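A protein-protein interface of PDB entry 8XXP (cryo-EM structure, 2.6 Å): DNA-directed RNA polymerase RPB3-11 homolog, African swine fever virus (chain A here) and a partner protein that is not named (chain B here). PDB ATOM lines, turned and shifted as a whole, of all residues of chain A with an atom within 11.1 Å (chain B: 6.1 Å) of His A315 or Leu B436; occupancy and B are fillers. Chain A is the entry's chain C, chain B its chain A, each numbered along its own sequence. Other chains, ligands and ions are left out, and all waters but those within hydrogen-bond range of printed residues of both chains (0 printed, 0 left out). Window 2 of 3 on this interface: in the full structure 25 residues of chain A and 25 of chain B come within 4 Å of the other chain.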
ATOM      1  N   ARG A 171      -8.799  -5.588  17.478  1.00  0.00           N
ATOM      2  CA  ARG A 171      -8.526  -4.218  17.882  1.00  0.00           C
ATOM      3  C   ARG A 171      -8.304  -4.082  19.379  1.00  0.00           C
ATOM      4  O   ARG A 171      -7.894  -3.009  19.831  1.00  0.00           O
ATOM      5  CB  ARG A 171      -9.658  -3.295  17.441  1.00  0.00           C
ATOM      6  CG  ARG A 171     -11.034  -3.841  17.696  1.00  0.00           C
ATOM      7  CD  ARG A 171     -12.084  -2.797  17.408  1.00  0.00           C
ATOM      8  NE  ARG A 171     -12.175  -1.823  18.485  1.00  0.00           N
ATOM      9  CZ  ARG A 171     -13.141  -1.799  19.393  1.00  0.00           C
ATOM     10  NH1 ARG A 171     -14.120  -2.686  19.383  1.00  0.00           N
ATOM     11  NH2 ARG A 171     -13.122  -0.862  20.333  1.00  0.00           N
ATOM     12  N   THR A 282     -24.016   8.733  20.631  1.00  0.00           N
ATOM     13  CA  THR A 282     -22.715   8.426  21.214  1.00  0.00           C
ATOM     14  C   THR A 282     -22.715   6.966  21.640  1.00  0.00           C
ATOM     15  O   THR A 282     -23.468   6.582  22.538  1.00  0.00           O
ATOM     16  CB  THR A 282     -22.421   9.335  22.406  1.00  0.00           C
ATOM     17  OG1 THR A 282     -22.473  10.704  21.993  1.00  0.00           O
ATOM     18  CG2 THR A 282     -21.051   9.046  22.973  1.00  0.00           C
ATOM     19  N   ILE A 283     -21.875   6.154  21.009  1.00  0.00           N
ATOM     20  CA  ILE A 283     -21.750   4.743  21.349  1.00  0.00           C
ATOM     21  C   ILE A 283     -20.325   4.489  21.807  1.00  0.00           C
ATOM     22  O   ILE A 283     -19.376   4.707  21.048  1.00  0.00           O
ATOM     23  CB  ILE A 283     -22.119   3.831  20.172  1.00  0.00           C
ATOM     24  CG1 ILE A 283     -23.597   3.984  19.836  1.00  0.00           C
ATOM     25  CG2 ILE A 283     -21.817   2.388  20.502  1.00  0.00           C
ATOM     26  CD1 ILE A 283     -23.835   4.643  18.531  1.00  0.00           C
ATOM     27  N   LYS A 284     -20.179   4.023  23.042  1.00  0.00           N
ATOM     28  CA  LYS A 284     -18.864   3.705  23.575  1.00  0.00           C
ATOM     29  C   LYS A 284     -18.293   2.471  22.897  1.00  0.00           C
ATOM     30  O   LYS A 284     -19.020   1.542  22.542  1.00  0.00           O
ATOM     31  CB  LYS A 284     -18.945   3.484  25.082  1.00  0.00           C
ATOM     32  CG  LYS A 284     -19.665   4.582  25.831  1.00  0.00           C
ATOM     33  CD  LYS A 284     -18.806   5.829  25.923  1.00  0.00           C
ATOM     34  CE  LYS A 284     -17.567   5.570  26.768  1.00  0.00           C
ATOM     35  NZ  LYS A 284     -16.905   6.827  27.216  1.00  0.00           N
ATOM     36  N   ASP A 285     -16.975   2.479  22.710  1.00  0.00           N
ATOM     37  CA  ASP A 285     -16.224   1.387  22.094  1.00  0.00           C
ATOM     38  C   ASP A 285     -16.645   1.125  20.656  1.00  0.00           C
ATOM     39  O   ASP A 285     -16.375   0.051  20.115  1.00  0.00           O
ATOM     40  CB  ASP A 285     -16.335   0.097  22.914  1.00  0.00           C
ATOM     41  CG  ASP A 285     -15.059  -0.714  22.897  1.00  0.00           C
ATOM     42  OD1 ASP A 285     -13.988  -0.132  22.627  1.00  0.00           O
ATOM     43  OD2 ASP A 285     -15.125  -1.935  23.147  1.00  0.00           O
ATOM     44  N   GLU A 286     -17.297   2.083  20.015  1.00  0.00           N
ATOM     45  CA  GLU A 286     -17.619   1.961  18.604  1.00  0.00           C
ATOM     46  C   GLU A 286     -16.527   2.620  17.780  1.00  0.00           C
ATOM     47  O   GLU A 286     -15.914   3.606  18.198  1.00  0.00           O
ATOM     48  CB  GLU A 286     -18.973   2.580  18.277  1.00  0.00           C
ATOM     49  CG  GLU A 286     -19.564   2.068  16.981  1.00  0.00           C
ATOM     50  CD  GLU A 286     -19.602   0.555  16.913  1.00  0.00           C
ATOM     51  OE1 GLU A 286     -20.539  -0.043  17.479  1.00  0.00           O
ATOM     52  OE2 GLU A 286     -18.698  -0.040  16.289  1.00  0.00           O
ATOM     53  N   THR A 287     -16.277   2.054  16.611  1.00  0.00           N
ATOM     54  CA  THR A 287     -15.126   2.395  15.801  1.00  0.00           C
ATOM     55  C   THR A 287     -15.563   3.133  14.542  1.00  0.00           C
ATOM     56  O   THR A 287     -16.731   3.487  14.375  1.00  0.00           O
ATOM     57  CB  THR A 287     -14.336   1.129  15.469  1.00  0.00           C
ATOM     58  OG1 THR A 287     -15.055   0.354  14.506  1.00  0.00           O
ATOM     59  CG2 THR A 287     -14.132   0.300  16.710  1.00  0.00           C
ATOM     60  N   HIS A 288     -14.599   3.375  13.655  1.00  0.00           N
ATOM     61  CA  HIS A 288     -14.866   4.079  12.412  1.00  0.00           C
ATOM     62  C   HIS A 288     -15.733   3.278  11.460  1.00  0.00           C
ATOM     63  O   HIS A 288     -16.332   3.864  10.560  1.00  0.00           O
ATOM     64  CB  HIS A 288     -13.555   4.428  11.717  1.00  0.00           C
ATOM     65  CG  HIS A 288     -12.761   5.472  12.425  1.00  0.00           C
ATOM     66  ND1 HIS A 288     -12.989   6.819  12.257  1.00  0.00           N
ATOM     67  CD2 HIS A 288     -11.736   5.371  13.301  1.00  0.00           C
ATOM     68  CE1 HIS A 288     -12.142   7.503  13.002  1.00  0.00           C
ATOM     69  NE2 HIS A 288     -11.372   6.648  13.646  1.00  0.00           N
ATOM     70  N   GLN A 311     -17.279  11.495  14.726  1.00  0.00           N
ATOM     71  CA  GLN A 311     -15.904  11.560  15.196  1.00  0.00           C
ATOM     72  C   GLN A 311     -15.625  10.367  16.094  1.00  0.00           C
ATOM     73  O   GLN A 311     -16.402  10.078  17.006  1.00  0.00           O
ATOM     74  CB  GLN A 311     -15.618  12.869  15.938  1.00  0.00           C
ATOM     75  CG  GLN A 311     -16.624  13.226  16.993  1.00  0.00           C
ATOM     76  CD  GLN A 311     -16.455  14.641  17.492  1.00  0.00           C
ATOM     77  OE1 GLN A 311     -15.354  15.188  17.479  1.00  0.00           O
ATOM     78  NE2 GLN A 311     -17.550  15.249  17.925  1.00  0.00           N
ATOM     79  N   CYS A 312     -14.533   9.668  15.815  1.00  0.00           N
ATOM     80  CA  CYS A 312     -14.007   8.627  16.688  1.00  0.00           C
ATOM     81  C   CYS A 312     -12.674   9.140  17.221  1.00  0.00           C
ATOM     82  O   CYS A 312     -11.612   8.841  16.682  1.00  0.00           O
ATOM     83  CB  CYS A 312     -13.834   7.299  15.956  1.00  0.00           C
ATOM     84  SG  CYS A 312     -15.338   6.431  15.557  1.00  0.00           S
ATOM     85  N   VAL A 313     -12.741   9.919  18.287  1.00  0.00           N
ATOM     86  CA  VAL A 313     -11.514  10.440  18.894  1.00  0.00           C
ATOM     87  C   VAL A 313     -10.725   9.276  19.479  1.00  0.00           C
ATOM     88  O   VAL A 313     -11.319   8.404  20.136  1.00  0.00           O
ATOM     89  CB  VAL A 313     -11.851  11.483  19.960  1.00  0.00           C
ATOM     90  CG1 VAL A 313     -10.599  12.065  20.543  1.00  0.00           C
ATOM     91  CG2 VAL A 313     -12.693  12.584  19.358  1.00  0.00           C
ATOM     92  N   PRO A 314      -9.420   9.173  19.220  1.00  0.00           N
ATOM     93  CA  PRO A 314      -8.667   8.034  19.765  1.00  0.00           C
ATOM     94  C   PRO A 314      -8.750   7.923  21.276  1.00  0.00           C
ATOM     95  O   PRO A 314      -8.858   6.808  21.798  1.00  0.00           O
ATOM     96  CB  PRO A 314      -7.243   8.305  19.271  1.00  0.00           C
ATOM     97  CG  PRO A 314      -7.443   9.044  18.008  1.00  0.00           C
ATOM     98  CD  PRO A 314      -8.632   9.926  18.233  1.00  0.00           C
ATOM     99  N   HIS A 315      -8.718   9.036  21.997  1.00  0.00           N
ATOM    100  CA  HIS A 315      -9.128   9.003  23.389  1.00  0.00           C
ATOM    101  C   HIS A 315     -10.636   9.229  23.463  1.00  0.00           C
ATOM    102  O   HIS A 315     -11.277   9.601  22.482  1.00  0.00           O
ATOM    103  CB  HIS A 315      -8.344  10.027  24.219  1.00  0.00           C
ATOM    104  CG  HIS A 315      -8.749  11.451  24.001  1.00  0.00           C
ATOM    105  ND1 HIS A 315      -8.269  12.215  22.960  1.00  0.00           N
ATOM    106  CD2 HIS A 315      -9.548  12.268  24.725  1.00  0.00           C
ATOM    107  CE1 HIS A 315      -8.779  13.431  23.036  1.00  0.00           C
ATOM    108  NE2 HIS A 315      -9.564  13.487  24.094  1.00  0.00           N
ATOM    109  N   LYS A 316     -11.203   8.960  24.635  1.00  0.00           N
ATOM    110  CA  LYS A 316     -12.647   8.941  24.878  1.00  0.00           C
ATOM    111  C   LYS A 316     -13.306   7.702  24.287  1.00  0.00           C
ATOM    112  O   LYS A 316     -14.467   7.424  24.598  1.00  0.00           O
ATOM    113  CB  LYS A 316     -13.341  10.198  24.335  1.00  0.00           C
ATOM    114  CG  LYS A 316     -12.765  11.494  24.849  1.00  0.00           C
ATOM    115  CD  LYS A 316     -13.786  12.609  24.862  1.00  0.00           C
ATOM    116  CE  LYS A 316     -14.185  13.017  23.463  1.00  0.00           C
ATOM    117  NZ  LYS A 316     -15.574  13.547  23.438  1.00  0.00           N
ATOM    118  N   GLN A 317     -12.571   6.950  23.470  1.00  0.00           N
ATOM    119  CA  GLN A 317     -12.943   5.607  23.017  1.00  0.00           C
ATOM    120  C   GLN A 317     -14.438   5.476  22.729  1.00  0.00           C
ATOM    121  O   GLN A 317     -15.128   4.606  23.261  1.00  0.00           O
ATOM    122  CB  GLN A 317     -12.495   4.560  24.034  1.00  0.00           C
ATOM    123  CG  GLN A 317     -11.043   4.702  24.481  1.00  0.00           C
ATOM    124  CD  GLN A 317     -10.894   4.758  25.991  1.00  0.00           C
ATOM    125  OE1 GLN A 317     -11.302   5.725  26.631  1.00  0.00           O
ATOM    126  NE2 GLN A 317     -10.306   3.717  26.565  1.00  0.00           N
ATOM    127  N   GLU A 318     -14.945   6.359  21.874  1.00  0.00           N
ATOM    128  CA  GLU A 318     -16.360   6.353  21.538  1.00  0.00           C
ATOM    129  C   GLU A 318     -16.546   6.895  20.132  1.00  0.00           C
ATOM    130  O   GLU A 318     -15.684   7.594  19.598  1.00  0.00           O
ATOM    131  CB  GLU A 318     -17.177   7.186  22.527  1.00  0.00           C
ATOM    132  CG  GLU A 318     -16.893   8.665  22.435  1.00  0.00           C
ATOM    133  CD  GLU A 318     -17.435   9.438  23.611  1.00  0.00           C
ATOM    134  OE1 GLU A 318     -17.883   8.798  24.582  1.00  0.00           O
ATOM    135  OE2 GLU A 318     -17.406  10.686  23.570  1.00  0.00           O
ATOM    136  N   MET A 319     -17.686   6.561  19.537  1.00  0.00           N
ATOM    137  CA  MET A 319     -18.122   7.135  18.272  1.00  0.00           C
ATOM    138  C   MET A 319     -19.259   8.104  18.554  1.00  0.00           C
ATOM    139  O   MET A 319     -20.252   7.731  19.184  1.00  0.00           O
ATOM    140  CB  MET A 319     -18.575   6.054  17.295  1.00  0.00           C
ATOM    141  CG  MET A 319     -18.722   6.534  15.861  1.00  0.00           C
ATOM    142  SD  MET A 319     -20.388   7.023  15.399  1.00  0.00           S
ATOM    143  CE  MET A 319     -21.351   5.792  16.259  1.00  0.00           C
ATOM    144  N   VAL A 320     -19.113   9.341  18.092  1.00  0.00           N
ATOM    145  CA  VAL A 320     -20.138  10.367  18.247  1.00  0.00           C
ATOM    146  C   VAL A 320     -20.605  10.769  16.859  1.00  0.00           C
ATOM    147  O   VAL A 320     -19.816  11.287  16.063  1.00  0.00           O
ATOM    148  CB  VAL A 320     -19.616  11.585  19.018  1.00  0.00           C
ATOM    149  CG1 VAL A 320     -20.619  12.705  18.953  1.00  0.00           C
ATOM    150  CG2 VAL A 320     -19.333  11.211  20.447  1.00  0.00           C
ATOM    151  N   ASN B 330      -1.537  15.752  20.874  1.00  0.00           N
ATOM    152  CA  ASN B 330      -2.909  15.269  20.757  1.00  0.00           C
ATOM    153  C   ASN B 330      -3.677  16.343  19.997  1.00  0.00           C
ATOM    154  O   ASN B 330      -4.084  17.349  20.579  1.00  0.00           O
ATOM    155  CB  ASN B 330      -3.520  14.999  22.122  1.00  0.00           C
ATOM    156  CG  ASN B 330      -4.814  14.235  22.039  1.00  0.00           C
ATOM    157  OD1 ASN B 330      -5.426  14.141  20.984  1.00  0.00           O
ATOM    158  ND2 ASN B 330      -5.243  13.685  23.162  1.00  0.00           N
ATOM    159  N   ASP B 332      -6.583  16.328  18.995  1.00  0.00           N
ATOM    160  CA  ASP B 332      -7.981  16.389  19.379  1.00  0.00           C
ATOM    161  C   ASP B 332      -8.203  17.138  20.681  1.00  0.00           C
ATOM    162  O   ASP B 332      -9.340  17.205  21.152  1.00  0.00           O
ATOM    163  CB  ASP B 332      -8.555  14.980  19.490  1.00  0.00           C
ATOM    164  CG  ASP B 332      -8.790  14.350  18.141  1.00  0.00           C
ATOM    165  OD1 ASP B 332      -9.578  14.910  17.353  1.00  0.00           O
ATOM    166  OD2 ASP B 332      -8.185  13.298  17.862  1.00  0.00           O
ATOM    167  N   LEU B 333      -7.156  17.697  21.271  1.00  0.00           N
ATOM    168  CA  LEU B 333      -7.276  18.513  22.465  1.00  0.00           C
ATOM    169  C   LEU B 333      -7.249  19.982  22.082  1.00  0.00           C
ATOM    170  O   LEU B 333      -6.463  20.396  21.229  1.00  0.00           O
ATOM    171  CB  LEU B 333      -6.148  18.220  23.453  1.00  0.00           C
ATOM    172  CG  LEU B 333      -6.184  16.895  24.202  1.00  0.00           C
ATOM    173  CD1 LEU B 333      -4.913  16.736  24.973  1.00  0.00           C
ATOM    174  CD2 LEU B 333      -7.370  16.846  25.128  1.00  0.00           C
ATOM    175  N   GLY B 339      -4.188  16.758  28.390  1.00  0.00           N
ATOM    176  CA  GLY B 339      -4.587  15.382  28.591  1.00  0.00           C
ATOM    177  C   GLY B 339      -3.951  14.779  29.822  1.00  0.00           C
ATOM    178  O   GLY B 339      -2.734  14.601  29.871  1.00  0.00           O
ATOM    179  N   TYR B 340      -4.759  14.462  30.826  1.00  0.00           N
ATOM    180  CA  TYR B 340      -4.248  13.967  32.096  1.00  0.00           C
ATOM    181  C   TYR B 340      -4.550  12.486  32.238  1.00  0.00           C
ATOM    182  O   TYR B 340      -5.727  12.111  32.331  1.00  0.00           O
ATOM    183  CB  TYR B 340      -4.865  14.749  33.254  1.00  0.00           C
ATOM    184  CG  TYR B 340      -3.996  14.801  34.484  1.00  0.00           C
ATOM    185  CD1 TYR B 340      -2.619  14.888  34.377  1.00  0.00           C
ATOM    186  CD2 TYR B 340      -4.553  14.771  35.751  1.00  0.00           C
ATOM    187  CE1 TYR B 340      -1.825  14.935  35.491  1.00  0.00           C
ATOM    188  CE2 TYR B 340      -3.766  14.822  36.871  1.00  0.00           C
ATOM    189  CZ  TYR B 340      -2.403  14.905  36.737  1.00  0.00           C
ATOM    190  OH  TYR B 340      -1.610  14.958  37.852  1.00  0.00           O
ATOM    191  N   PRO B 341      -3.547  11.611  32.258  1.00  0.00           N
ATOM    192  CA  PRO B 341      -3.824  10.181  32.417  1.00  0.00           C
ATOM    193  C   PRO B 341      -4.527   9.889  33.734  1.00  0.00           C
ATOM    194  O   PRO B 341      -4.271  10.525  34.756  1.00  0.00           O
ATOM    195  CB  PRO B 341      -2.433   9.542  32.361  1.00  0.00           C
ATOM    196  CG  PRO B 341      -1.489  10.644  32.635  1.00  0.00           C
ATOM    197  CD  PRO B 341      -2.112  11.872  32.084  1.00  0.00           C
ATOM    198  N   ILE B 342      -5.424   8.902  33.694  1.00  0.00           N
ATOM    199  CA  ILE B 342      -6.331   8.662  34.810  1.00  0.00           C
ATOM    200  C   ILE B 342      -5.580   8.221  36.059  1.00  0.00           C
ATOM    201  O   ILE B 342      -6.025   8.490  37.178  1.00  0.00           O
ATOM    202  CB  ILE B 342      -7.413   7.641  34.412  1.00  0.00           C
ATOM    203  CG1 ILE B 342      -8.453   7.516  35.527  1.00  0.00           C
ATOM    204  CG2 ILE B 342      -6.795   6.297  34.087  1.00  0.00           C
ATOM    205  CD1 ILE B 342      -9.669   6.736  35.145  1.00  0.00           C
ATOM    206  N   SER B 343      -4.445   7.539  35.904  1.00  0.00           N
ATOM    207  CA  SER B 343      -3.680   7.122  37.074  1.00  0.00           C
ATOM    208  C   SER B 343      -3.211   8.325  37.876  1.00  0.00           C
ATOM    209  O   SER B 343      -3.255   8.313  39.111  1.00  0.00           O
ATOM    210  CB  SER B 343      -2.491   6.267  36.648  1.00  0.00           C
ATOM    211  OG  SER B 343      -1.700   6.939  35.689  1.00  0.00           O
ATOM    212  N   THR B 411     -12.456  15.663  34.313  1.00  0.00           N
ATOM    213  CA  THR B 411     -12.347  16.493  33.123  1.00  0.00           C
ATOM    214  C   THR B 411     -13.041  17.827  33.360  1.00  0.00           C
ATOM    215  O   THR B 411     -14.156  17.878  33.883  1.00  0.00           O
ATOM    216  CB  THR B 411     -12.951  15.779  31.916  1.00  0.00           C
ATOM    217  OG1 THR B 411     -12.172  14.620  31.614  1.00  0.00           O
ATOM    218  CG2 THR B 411     -12.950  16.681  30.708  1.00  0.00           C
ATOM    219  N   VAL B 434      -8.321  17.319  30.654  1.00  0.00           N
ATOM    220  CA  VAL B 434      -9.044  16.248  29.981  1.00  0.00           C
ATOM    221  C   VAL B 434      -8.447  14.943  30.479  1.00  0.00           C
ATOM    222  O   VAL B 434      -7.293  14.627  30.174  1.00  0.00           O
ATOM    223  CB  VAL B 434      -8.951  16.355  28.455  1.00  0.00           C
ATOM    224  CG1 VAL B 434      -9.606  15.158  27.812  1.00  0.00           C
ATOM    225  CG2 VAL B 434      -9.601  17.625  27.981  1.00  0.00           C
ATOM    226  N   VAL B 435      -9.218  14.183  31.245  1.00  0.00           N
ATOM    227  CA  VAL B 435      -8.705  12.949  31.826  1.00  0.00           C
ATOM    228  C   VAL B 435      -8.754  11.849  30.779  1.00  0.00           C
ATOM    229  O   VAL B 435      -9.815  11.550  30.223  1.00  0.00           O
ATOM    230  CB  VAL B 435      -9.485  12.554  33.085  1.00  0.00           C
ATOM    231  CG1 VAL B 435      -9.021  11.203  33.567  1.00  0.00           C
ATOM    232  CG2 VAL B 435      -9.278  13.588  34.164  1.00  0.00           C
ATOM    233  N   LEU B 436      -7.603  11.247  30.507  1.00  0.00           N
ATOM    234  CA  LEU B 436      -7.488  10.158  29.546  1.00  0.00           C
ATOM    235  C   LEU B 436      -7.743   8.855  30.286  1.00  0.00           C
ATOM    236  O   LEU B 436      -6.893   8.379  31.038  1.00  0.00           O
ATOM    237  CB  LEU B 436      -6.118  10.173  28.886  1.00  0.00           C
ATOM    238  CG  LEU B 436      -5.675  11.543  28.386  1.00  0.00           C
ATOM    239  CD1 LEU B 436      -4.198  11.542  28.116  1.00  0.00           C
ATOM    240  CD2 LEU B 436      -6.446  11.933  27.147  1.00  0.00           C
ATOM    241  N   GLU B 437      -8.916   8.273  30.068  1.00  0.00           N
ATOM    242  CA  GLU B 437      -9.325   7.089  30.805  1.00  0.00           C
ATOM    243  C   GLU B 437      -8.698   5.810  30.273  1.00  0.00           C
ATOM    244  O   GLU B 437      -8.902   4.749  30.870  1.00  0.00           O
ATOM    245  CB  GLU B 437     -10.848   6.977  30.803  1.00  0.00           C
ATOM    246  CG  GLU B 437     -11.501   7.872  31.840  1.00  0.00           C
ATOM    247  CD  GLU B 437     -12.918   8.269  31.478  1.00  0.00           C
ATOM    248  OE1 GLU B 437     -13.285   8.166  30.291  1.00  0.00           O
ATOM    249  OE2 GLU B 437     -13.663   8.690  32.384  1.00  0.00           O
ATOM    250  N   ASN B 438      -7.952   5.879  29.185  1.00  0.00           N
ATOM    251  CA  ASN B 438      -7.154   4.746  28.741  1.00  0.00           C
ATOM    252  C   ASN B 438      -6.046   4.493  29.753  1.00  0.00           C
ATOM    253  O   ASN B 438      -5.213   5.380  29.977  1.00  0.00           O
ATOM    254  CB  ASN B 438      -6.566   5.036  27.365  1.00  0.00           C
ATOM    255  CG  ASN B 438      -5.914   3.826  26.733  1.00  0.00           C
ATOM    256  OD1 ASN B 438      -5.703   2.808  27.380  1.00  0.00           O
ATOM    257  ND2 ASN B 438      -5.585   3.940  25.457  1.00  0.00           N
ATOM    258  N   PRO B 439      -5.990   3.318  30.384  1.00  0.00           N
ATOM    259  CA  PRO B 439      -4.958   3.083  31.403  1.00  0.00           C
ATOM    260  C   PRO B 439      -3.562   2.920  30.836  1.00  0.00           C
ATOM    261  O   PRO B 439      -2.590   3.023  31.593  1.00  0.00           O
ATOM    262  CB  PRO B 439      -5.433   1.798  32.086  1.00  0.00           C
ATOM    263  CG  PRO B 439      -6.218   1.104  31.045  1.00  0.00           C
ATOM    264  CD  PRO B 439      -6.905   2.173  30.257  1.00  0.00           C
ATOM    265  N   ILE B 441      -2.087   4.897  28.676  1.00  0.00           N
ATOM    266  CA  ILE B 441      -1.478   6.186  28.378  1.00  0.00           C
ATOM    267  C   ILE B 441      -0.988   6.789  29.685  1.00  0.00           C
ATOM    268  O   ILE B 441      -1.742   6.874  30.659  1.00  0.00           O
ATOM    269  CB  ILE B 441      -2.476   7.122  27.674  1.00  0.00           C
ATOM    270  CG1 ILE B 441      -2.445   6.941  26.154  1.00  0.00           C
ATOM    271  CG2 ILE B 441      -2.145   8.564  27.975  1.00  0.00           C
ATOM    272  CD1 ILE B 441      -2.574   5.527  25.670  1.00  0.00           C
ATOM    273  N   THR B 443       1.284   9.721  29.449  1.00  0.00           N
ATOM    274  CA  THR B 443       1.889  10.985  29.065  1.00  0.00           C
ATOM    275  C   THR B 443       0.932  12.141  29.305  1.00  0.00           C
ATOM    276  O   THR B 443      -0.287  11.978  29.343  1.00  0.00           O
ATOM    277  CB  THR B 443       2.296  10.969  27.593  1.00  0.00           C
ATOM    278  OG1 THR B 443       1.278  10.332  26.821  1.00  0.00           O
ATOM    279  CG2 THR B 443       3.578  10.232  27.413  1.00  0.00           C
ATOM    280  N   PHE B 444       1.510  13.324  29.461  1.00  0.00           N
ATOM    281  CA  PHE B 444       0.741  14.556  29.412  1.00  0.00           C
ATOM    282  C   PHE B 444       0.501  14.900  27.951  1.00  0.00           C
ATOM    283  O   PHE B 444       1.452  15.041  27.182  1.00  0.00           O
ATOM    284  CB  PHE B 444       1.487  15.686  30.114  1.00  0.00           C
ATOM    285  CG  PHE B 444       1.626  15.503  31.595  1.00  0.00           C
ATOM    286  CD1 PHE B 444       0.835  14.603  32.276  1.00  0.00           C
ATOM    287  CD2 PHE B 444       2.541  16.244  32.306  1.00  0.00           C
ATOM    288  CE1 PHE B 444       0.968  14.444  33.630  1.00  0.00           C
ATOM    289  CE2 PHE B 444       2.671  16.089  33.655  1.00  0.00           C
ATOM    290  CZ  PHE B 444       1.885  15.191  34.320  1.00  0.00           C
ATOM    291  N   GLN B 445      -0.754  15.011  27.555  1.00  0.00           N
ATOM    292  CA  GLN B 445      -1.084  15.261  26.162  1.00  0.00           C
ATOM    293  C   GLN B 445      -1.551  16.696  25.986  1.00  0.00           C
ATOM    294  O   GLN B 445      -2.319  17.218  26.796  1.00  0.00           O
ATOM    295  CB  GLN B 445      -2.148  14.285  25.674  1.00  0.00           C
ATOM    296  CG  GLN B 445      -1.768  12.854  25.920  1.00  0.00           C
ATOM    297  CD  GLN B 445      -2.320  11.918  24.889  1.00  0.00           C
ATOM    298  OE1 GLN B 445      -3.411  12.128  24.367  1.00  0.00           O
ATOM    299  NE2 GLN B 445      -1.577  10.866  24.591  1.00  0.00           N
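A ring nitrogen (ND1) of His A315 lies within hydrogen-bond range of the side-chain amide nitrogen of Asn B330.
Val A313 touches Asp B332. Asp B332 touches Pro A314. His A315 touches Asp B332 (CE1 to CB, 3.9 Å). Leu B436 touches His A315 (CD2 to CG, 3.9 Å). Gln A317 touches Asn B438 (NE2 to CA, 3.97 Å).
Of the printed residues of chain B, Val A313 touches Asp B332 (3.7 Å). Of the printed residues of chain B, Pro A314 touches Asp B332. Of the printed residues of chain B, Gln A317 touches Asn B438 (3.97 Å). Printed residues of chain A within 4 Å of Asn B330: His A315. Asp B332 touches just these residues of chain A: Val A313 (3.7 Å), Pro A314 (3.4 Å) and His A315 (3.9 Å). No residue of chain A comes within 4 Å of Gly B339. Pro B341 touches none of the printed residues of chain A. No residue of chain A comes within 4 Å of Ile B342. No residue of chain A comes within 4 Å of Val B434. No residue of chain A comes within 4 Å of Val B435. Of chain A, only His A315 comes within 4 Å of Leu B436. No residue of chain A comes within 4 Å of Glu B437. Asn B438 touches one residue of chain A. Gln B445 touches none of the printed residues of chain A. The nearest residue of chain A that does not touch Leu B436 is Gln A317 (6.0 Å). The nearest printed residue of chain B that does not touch Pro A314 is Asn B438 (5.7 Å).
OD1 of Asn B330 lies close to N of Asp B332 (3.2 Å). OE1 of Gln B445 sits at hydrogen-bond distance from ND2 of Asn B330, 2.7 Å away. O of Tyr B340 is in hydrogen-bond range of N of Leu B436 (2.8 Å). The backbone NH of Ile B342 is in hydrogen-bond range of the backbone carbonyl oxygen of Leu B436, at 3.1 Å. O of Gln A317 is in hydrogen-bond range of N of Asp A285, 2.9 Å away.
Printed residues of chain B that touch a printed residue of chain A: Asn B330, Asp B332, Leu B436 and Asn B438. Hydrophobic or aromatic side chains of chain B within 4 Å of the printed part of chain A: Leu B436. Of the 18 printed residues of chain A, 4 touch a printed residue of chain B. Printed residues of chain A that touch a printed residue of chain B: Val A313, Pro A314, His A315 and Gln A317. Hydrophobic or aromatic side chains of chain A within 4 Å of the printed part of chain B: Val A313, Pro A314 and His A315. Among the printed residues, 6 pairs touch across the chains. Among the printed residues, no Asp or Glu carboxylate lies within 4 Å of a Lys or Arg side-chain nitrogen of the other chain.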
